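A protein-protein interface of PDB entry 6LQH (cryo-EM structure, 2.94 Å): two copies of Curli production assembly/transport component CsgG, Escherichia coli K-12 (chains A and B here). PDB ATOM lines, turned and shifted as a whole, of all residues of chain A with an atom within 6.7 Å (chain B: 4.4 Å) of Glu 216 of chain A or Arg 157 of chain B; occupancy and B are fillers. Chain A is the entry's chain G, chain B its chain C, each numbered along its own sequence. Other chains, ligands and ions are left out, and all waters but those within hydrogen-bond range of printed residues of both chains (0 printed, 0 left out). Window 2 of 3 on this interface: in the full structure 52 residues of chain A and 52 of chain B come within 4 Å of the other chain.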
ATOM      1  N   GLY A 204      13.099  17.402 -15.476  1.00  0.00           N
ATOM      2  CA  GLY A 204      12.474  18.664 -15.151  1.00  0.00           C
ATOM      3  C   GLY A 204      13.072  19.860 -15.856  1.00  0.00           C
ATOM      4  O   GLY A 204      14.254  19.868 -16.197  1.00  0.00           O
ATOM      5  N   VAL A 205      12.247  20.874 -16.080  1.00  0.00           N
ATOM      6  CA  VAL A 205      12.658  22.131 -16.688  1.00  0.00           C
ATOM      7  C   VAL A 205      12.268  23.261 -15.751  1.00  0.00           C
ATOM      8  O   VAL A 205      11.150  23.281 -15.229  1.00  0.00           O
ATOM      9  CB  VAL A 205      12.010  22.333 -18.071  1.00  0.00           C
ATOM     10  CG1 VAL A 205      12.678  23.477 -18.799  1.00  0.00           C
ATOM     11  CG2 VAL A 205      12.090  21.061 -18.882  1.00  0.00           C
ATOM     12  N   PHE A 206      13.191  24.191 -15.520  1.00  0.00           N
ATOM     13  CA  PHE A 206      12.864  25.361 -14.715  1.00  0.00           C
ATOM     14  C   PHE A 206      13.505  26.626 -15.265  1.00  0.00           C
ATOM     15  O   PHE A 206      13.897  27.505 -14.496  1.00  0.00           O
ATOM     16  CB  PHE A 206      13.270  25.167 -13.256  1.00  0.00           C
ATOM     17  CG  PHE A 206      12.381  25.887 -12.282  1.00  0.00           C
ATOM     18  CD1 PHE A 206      11.258  25.270 -11.766  1.00  0.00           C
ATOM     19  CD2 PHE A 206      12.666  27.180 -11.884  1.00  0.00           C
ATOM     20  CE1 PHE A 206      10.443  25.930 -10.874  1.00  0.00           C
ATOM     21  CE2 PHE A 206      11.852  27.844 -10.999  1.00  0.00           C
ATOM     22  CZ  PHE A 206      10.741  27.220 -10.492  1.00  0.00           C
ATOM     23  N   ARG A 207      13.644  26.739 -16.576  1.00  0.00           N
ATOM     24  CA  ARG A 207      14.298  27.914 -17.117  1.00  0.00           C
ATOM     25  C   ARG A 207      13.263  28.948 -17.552  1.00  0.00           C
ATOM     26  O   ARG A 207      12.053  28.727 -17.480  1.00  0.00           O
ATOM     27  CB  ARG A 207      15.229  27.526 -18.262  1.00  0.00           C
ATOM     28  CG  ARG A 207      14.556  26.901 -19.459  1.00  0.00           C
ATOM     29  CD  ARG A 207      15.606  26.439 -20.454  1.00  0.00           C
ATOM     30  NE  ARG A 207      15.103  26.421 -21.821  1.00  0.00           N
ATOM     31  CZ  ARG A 207      15.255  27.420 -22.684  1.00  0.00           C
ATOM     32  NH1 ARG A 207      15.892  28.521 -22.318  1.00  0.00           N
ATOM     33  NH2 ARG A 207      14.764  27.320 -23.912  1.00  0.00           N
ATOM     34  N   LEU A 214       8.328  32.155 -17.060  1.00  0.00           N
ATOM     35  CA  LEU A 214       9.028  31.014 -16.489  1.00  0.00           C
ATOM     36  C   LEU A 214       8.252  29.747 -16.807  1.00  0.00           C
ATOM     37  O   LEU A 214       7.074  29.633 -16.456  1.00  0.00           O
ATOM     38  CB  LEU A 214       9.184  31.186 -14.979  1.00  0.00           C
ATOM     39  CG  LEU A 214       9.754  30.020 -14.183  1.00  0.00           C
ATOM     40  CD1 LEU A 214      11.254  29.960 -14.350  1.00  0.00           C
ATOM     41  CD2 LEU A 214       9.388  30.176 -12.728  1.00  0.00           C
ATOM     42  N   LEU A 215       8.911  28.797 -17.463  1.00  0.00           N
ATOM     43  CA  LEU A 215       8.313  27.506 -17.786  1.00  0.00           C
ATOM     44  C   LEU A 215       8.902  26.435 -16.880  1.00  0.00           C
ATOM     45  O   LEU A 215      10.083  26.097 -16.994  1.00  0.00           O
ATOM     46  CB  LEU A 215       8.535  27.150 -19.249  1.00  0.00           C
ATOM     47  CG  LEU A 215       8.104  25.743 -19.638  1.00  0.00           C
ATOM     48  CD1 LEU A 215       7.200  25.818 -20.835  1.00  0.00           C
ATOM     49  CD2 LEU A 215       9.312  24.896 -19.948  1.00  0.00           C
ATOM     50  N   GLU A 216       8.071  25.895 -15.998  1.00  0.00           N
ATOM     51  CA  GLU A 216       8.428  24.778 -15.144  1.00  0.00           C
ATOM     52  C   GLU A 216       7.742  23.519 -15.647  1.00  0.00           C
ATOM     53  O   GLU A 216       6.629  23.560 -16.173  1.00  0.00           O
ATOM     54  CB  GLU A 216       8.031  25.042 -13.696  1.00  0.00           C
ATOM     55  CG  GLU A 216       8.088  26.505 -13.335  1.00  0.00           C
ATOM     56  CD  GLU A 216       7.324  26.832 -12.080  1.00  0.00           C
ATOM     57  OE1 GLU A 216       6.955  25.898 -11.336  1.00  0.00           O
ATOM     58  OE2 GLU A 216       7.075  28.032 -11.840  1.00  0.00           O
ATOM     59  N   GLY A 217       8.421  22.396 -15.482  1.00  0.00           N
ATOM     60  CA  GLY A 217       7.905  21.133 -15.953  1.00  0.00           C
ATOM     61  C   GLY A 217       8.603  19.990 -15.264  1.00  0.00           C
ATOM     62  O   GLY A 217       9.764  20.113 -14.883  1.00  0.00           O
ATOM     63  N   GLU A 218       7.914  18.871 -15.114  1.00  0.00           N
ATOM     64  CA  GLU A 218       8.455  17.756 -14.362  1.00  0.00           C
ATOM     65  C   GLU A 218       7.780  16.485 -14.836  1.00  0.00           C
ATOM     66  O   GLU A 218       6.562  16.454 -15.003  1.00  0.00           O
ATOM     67  CB  GLU A 218       8.228  17.952 -12.865  1.00  0.00           C
ATOM     68  CG  GLU A 218       8.582  16.756 -12.030  1.00  0.00           C
ATOM     69  CD  GLU A 218       9.880  16.925 -11.271  1.00  0.00           C
ATOM     70  OE1 GLU A 218       9.825  16.869 -10.028  1.00  0.00           O
ATOM     71  OE2 GLU A 218      10.944  17.112 -11.898  1.00  0.00           O
ATOM     72  N   GLY B 155       3.984  17.126 -14.344  1.00  0.00           N
ATOM     73  CA  GLY B 155       3.446  18.427 -14.028  1.00  0.00           C
ATOM     74  C   GLY B 155       4.105  19.525 -14.824  1.00  0.00           C
ATOM     75  O   GLY B 155       5.319  19.706 -14.745  1.00  0.00           O
ATOM     76  N   ALA B 156       3.322  20.264 -15.594  1.00  0.00           N
ATOM     77  CA  ALA B 156       3.831  21.388 -16.357  1.00  0.00           C
ATOM     78  C   ALA B 156       3.332  22.681 -15.739  1.00  0.00           C
ATOM     79  O   ALA B 156       2.359  22.687 -14.985  1.00  0.00           O
ATOM     80  CB  ALA B 156       3.399  21.314 -17.819  1.00  0.00           C
ATOM     81  N   ARG B 157       4.014  23.776 -16.044  1.00  0.00           N
ATOM     82  CA  ARG B 157       3.599  25.078 -15.538  1.00  0.00           C
ATOM     83  C   ARG B 157       4.196  26.152 -16.427  1.00  0.00           C
ATOM     84  O   ARG B 157       5.400  26.407 -16.367  1.00  0.00           O
ATOM     85  CB  ARG B 157       4.035  25.268 -14.095  1.00  0.00           C
ATOM     86  CG  ARG B 157       3.558  26.551 -13.481  1.00  0.00           C
ATOM     87  CD  ARG B 157       3.599  26.471 -11.976  1.00  0.00           C
ATOM     88  NE  ARG B 157       3.641  27.796 -11.371  1.00  0.00           N
ATOM     89  CZ  ARG B 157       2.584  28.414 -10.859  1.00  0.00           C
ATOM     90  NH1 ARG B 157       1.399  27.822 -10.873  1.00  0.00           N
ATOM     91  NH2 ARG B 157       2.714  29.620 -10.328  1.00  0.00           N
ATOM     92  N   TYR B 158       3.368  26.781 -17.238  1.00  0.00           N
ATOM     93  CA  TYR B 158       3.798  27.949 -17.984  1.00  0.00           C
ATOM     94  C   TYR B 158       3.601  29.177 -17.096  1.00  0.00           C
ATOM     95  O   TYR B 158       3.449  29.055 -15.880  1.00  0.00           O
ATOM     96  CB  TYR B 158       3.062  28.035 -19.322  1.00  0.00           C
ATOM     97  CG  TYR B 158       3.651  29.088 -20.226  1.00  0.00           C
ATOM     98  CD1 TYR B 158       5.018  29.175 -20.410  1.00  0.00           C
ATOM     99  CD2 TYR B 158       2.845  30.019 -20.860  1.00  0.00           C
ATOM    100  CE1 TYR B 158       5.566  30.143 -21.216  1.00  0.00           C
ATOM    101  CE2 TYR B 158       3.386  30.992 -21.670  1.00  0.00           C
ATOM    102  CZ  TYR B 158       4.747  31.048 -21.845  1.00  0.00           C
ATOM    103  OH  TYR B 158       5.293  32.016 -22.653  1.00  0.00           O
ATOM    104  N   GLY B 160       2.380  31.466 -14.836  1.00  0.00           N
ATOM    105  CA  GLY B 160       1.225  31.440 -13.964  1.00  0.00           C
ATOM    106  C   GLY B 160       0.481  30.122 -13.958  1.00  0.00           C
ATOM    107  O   GLY B 160       0.458  29.422 -12.944  1.00  0.00           O
ATOM    108  N   ILE B 161      -0.123  29.769 -15.091  1.00  0.00           N
ATOM    109  CA  ILE B 161      -0.997  28.603 -15.159  1.00  0.00           C
ATOM    110  C   ILE B 161      -0.158  27.334 -15.122  1.00  0.00           C
ATOM    111  O   ILE B 161       0.774  27.165 -15.914  1.00  0.00           O
ATOM    112  CB  ILE B 161      -1.874  28.642 -16.415  1.00  0.00           C
ATOM    113  CG1 ILE B 161      -2.599  29.983 -16.539  1.00  0.00           C
ATOM    114  CG2 ILE B 161      -2.864  27.501 -16.398  1.00  0.00           C
ATOM    115  CD1 ILE B 161      -1.858  31.023 -17.353  1.00  0.00           C
ATOM    116  N   GLY B 162      -0.496  26.429 -14.210  1.00  0.00           N
ATOM    117  CA  GLY B 162       0.182  25.155 -14.125  1.00  0.00           C
ATOM    118  C   GLY B 162      -0.801  24.050 -13.801  1.00  0.00           C
ATOM    119  O   GLY B 162      -1.925  24.302 -13.370  1.00  0.00           O
ATOM    120  N   GLY B 204      -3.575  25.173 -11.167  1.00  0.00           N
ATOM    121  CA  GLY B 204      -3.486  26.398 -10.406  1.00  0.00           C
ATOM    122  C   GLY B 204      -2.999  27.592 -11.194  1.00  0.00           C
ATOM    123  O   GLY B 204      -2.246  27.451 -12.157  1.00  0.00           O
ATOM    124  N   PHE B 206      -1.323  31.547 -10.531  1.00  0.00           N
ATOM    125  CA  PHE B 206      -0.778  32.494  -9.567  1.00  0.00           C
ATOM    126  C   PHE B 206      -0.153  33.701 -10.250  1.00  0.00           C
ATOM    127  O   PHE B 206       0.846  34.237  -9.766  1.00  0.00           O
ATOM    128  CB  PHE B 206       0.247  31.830  -8.651  1.00  0.00           C
ATOM    129  CG  PHE B 206       0.294  32.422  -7.270  1.00  0.00           C
ATOM    130  CD1 PHE B 206      -0.517  31.933  -6.267  1.00  0.00           C
ATOM    131  CD2 PHE B 206       1.147  33.472  -6.979  1.00  0.00           C
ATOM    132  CE1 PHE B 206      -0.474  32.476  -5.002  1.00  0.00           C
ATOM    133  CE2 PHE B 206       1.190  34.021  -5.721  1.00  0.00           C
ATOM    134  CZ  PHE B 206       0.380  33.524  -4.730  1.00  0.00           C
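The side-chain carboxylate (OE2) of Glu 216 of chain A is in salt-bridge range of the guanidinium group (NE) of Arg 157 of chain B (3.5 Å). The backbone NH of Gly 155 of chain B lies within hydrogen-bond range of the backbone carbonyl oxygen of Glu 218 of chain A (2.7 Å).
The guanidinium group (NH1) of Arg 157 of chain B is in hydrogen-bond range of the backbone carbonyl oxygen (O) of Gly 160 of chain B (2.8 Å). O of Arg 207 of chain A is in hydrogen-bond range of N of Leu 215 of chain A (3.1 Å). The backbone carbonyl oxygen (O) of Gly 217 of chain A lies within hydrogen-bond range of the backbone NH (N) of Val 205 of chain A, 2.9 Å away.
Printed residues of chain B that touch a printed residue of chain A: Gly 155, Ala 156, Arg 157 and Tyr 158. Along chain B the printed residues that touch a printed residue of chain A span positions 155 to 158. Of the 9 printed residues of chain A, 5 touch a printed residue of chain B. Printed residues of chain A that touch a printed residue of chain B: Leu 214, Leu 215, Glu 216, Gly 217 and Glu 218.
Of chain B, only Ala 156 and Arg 157 come within 4 Å of Glu 216 of chain A. Arg 157 of chain B touches just these residues of chain A: Leu 214, Leu 215 and Glu 216. Of the printed residues of chain B, Leu 214 of chain A touches Arg 157 and Tyr 158. Of the printed residues of chain B, Gly 217 of chain A touches Gly 155. Printed residues of chain A within 4 Å of Tyr 158 of chain B: Leu 214. Of the printed residues of chain A, Ala 156 of chain B touches Glu 216. Of the printed residues of chain B, Leu 215 of chain A touches Arg 157 (3.4 Å). Gly 204 of chain B touches none of the printed residues of chain A. The nearest printed residue of chain A that does not touch Tyr 158 of chain B is Leu 215 of chain A (4.03 Å).
Among the printed residues, merely in contact across the chains: Leu 214 of chain A with Arg 157 of chain B, Leu 214 of chain A with Tyr 158 of chain B, Leu 215 of chain A with Arg 157 of chain B, Glu 216 of chain A with Ala 156 of chain B and Gly 217 of chain A with Gly 155 of chain B.
Positions printed for both chains: 204 and 206. Of the 7 pairs that touch across the chains among the printed residues, none has its exchanged pair printed and touching as well.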
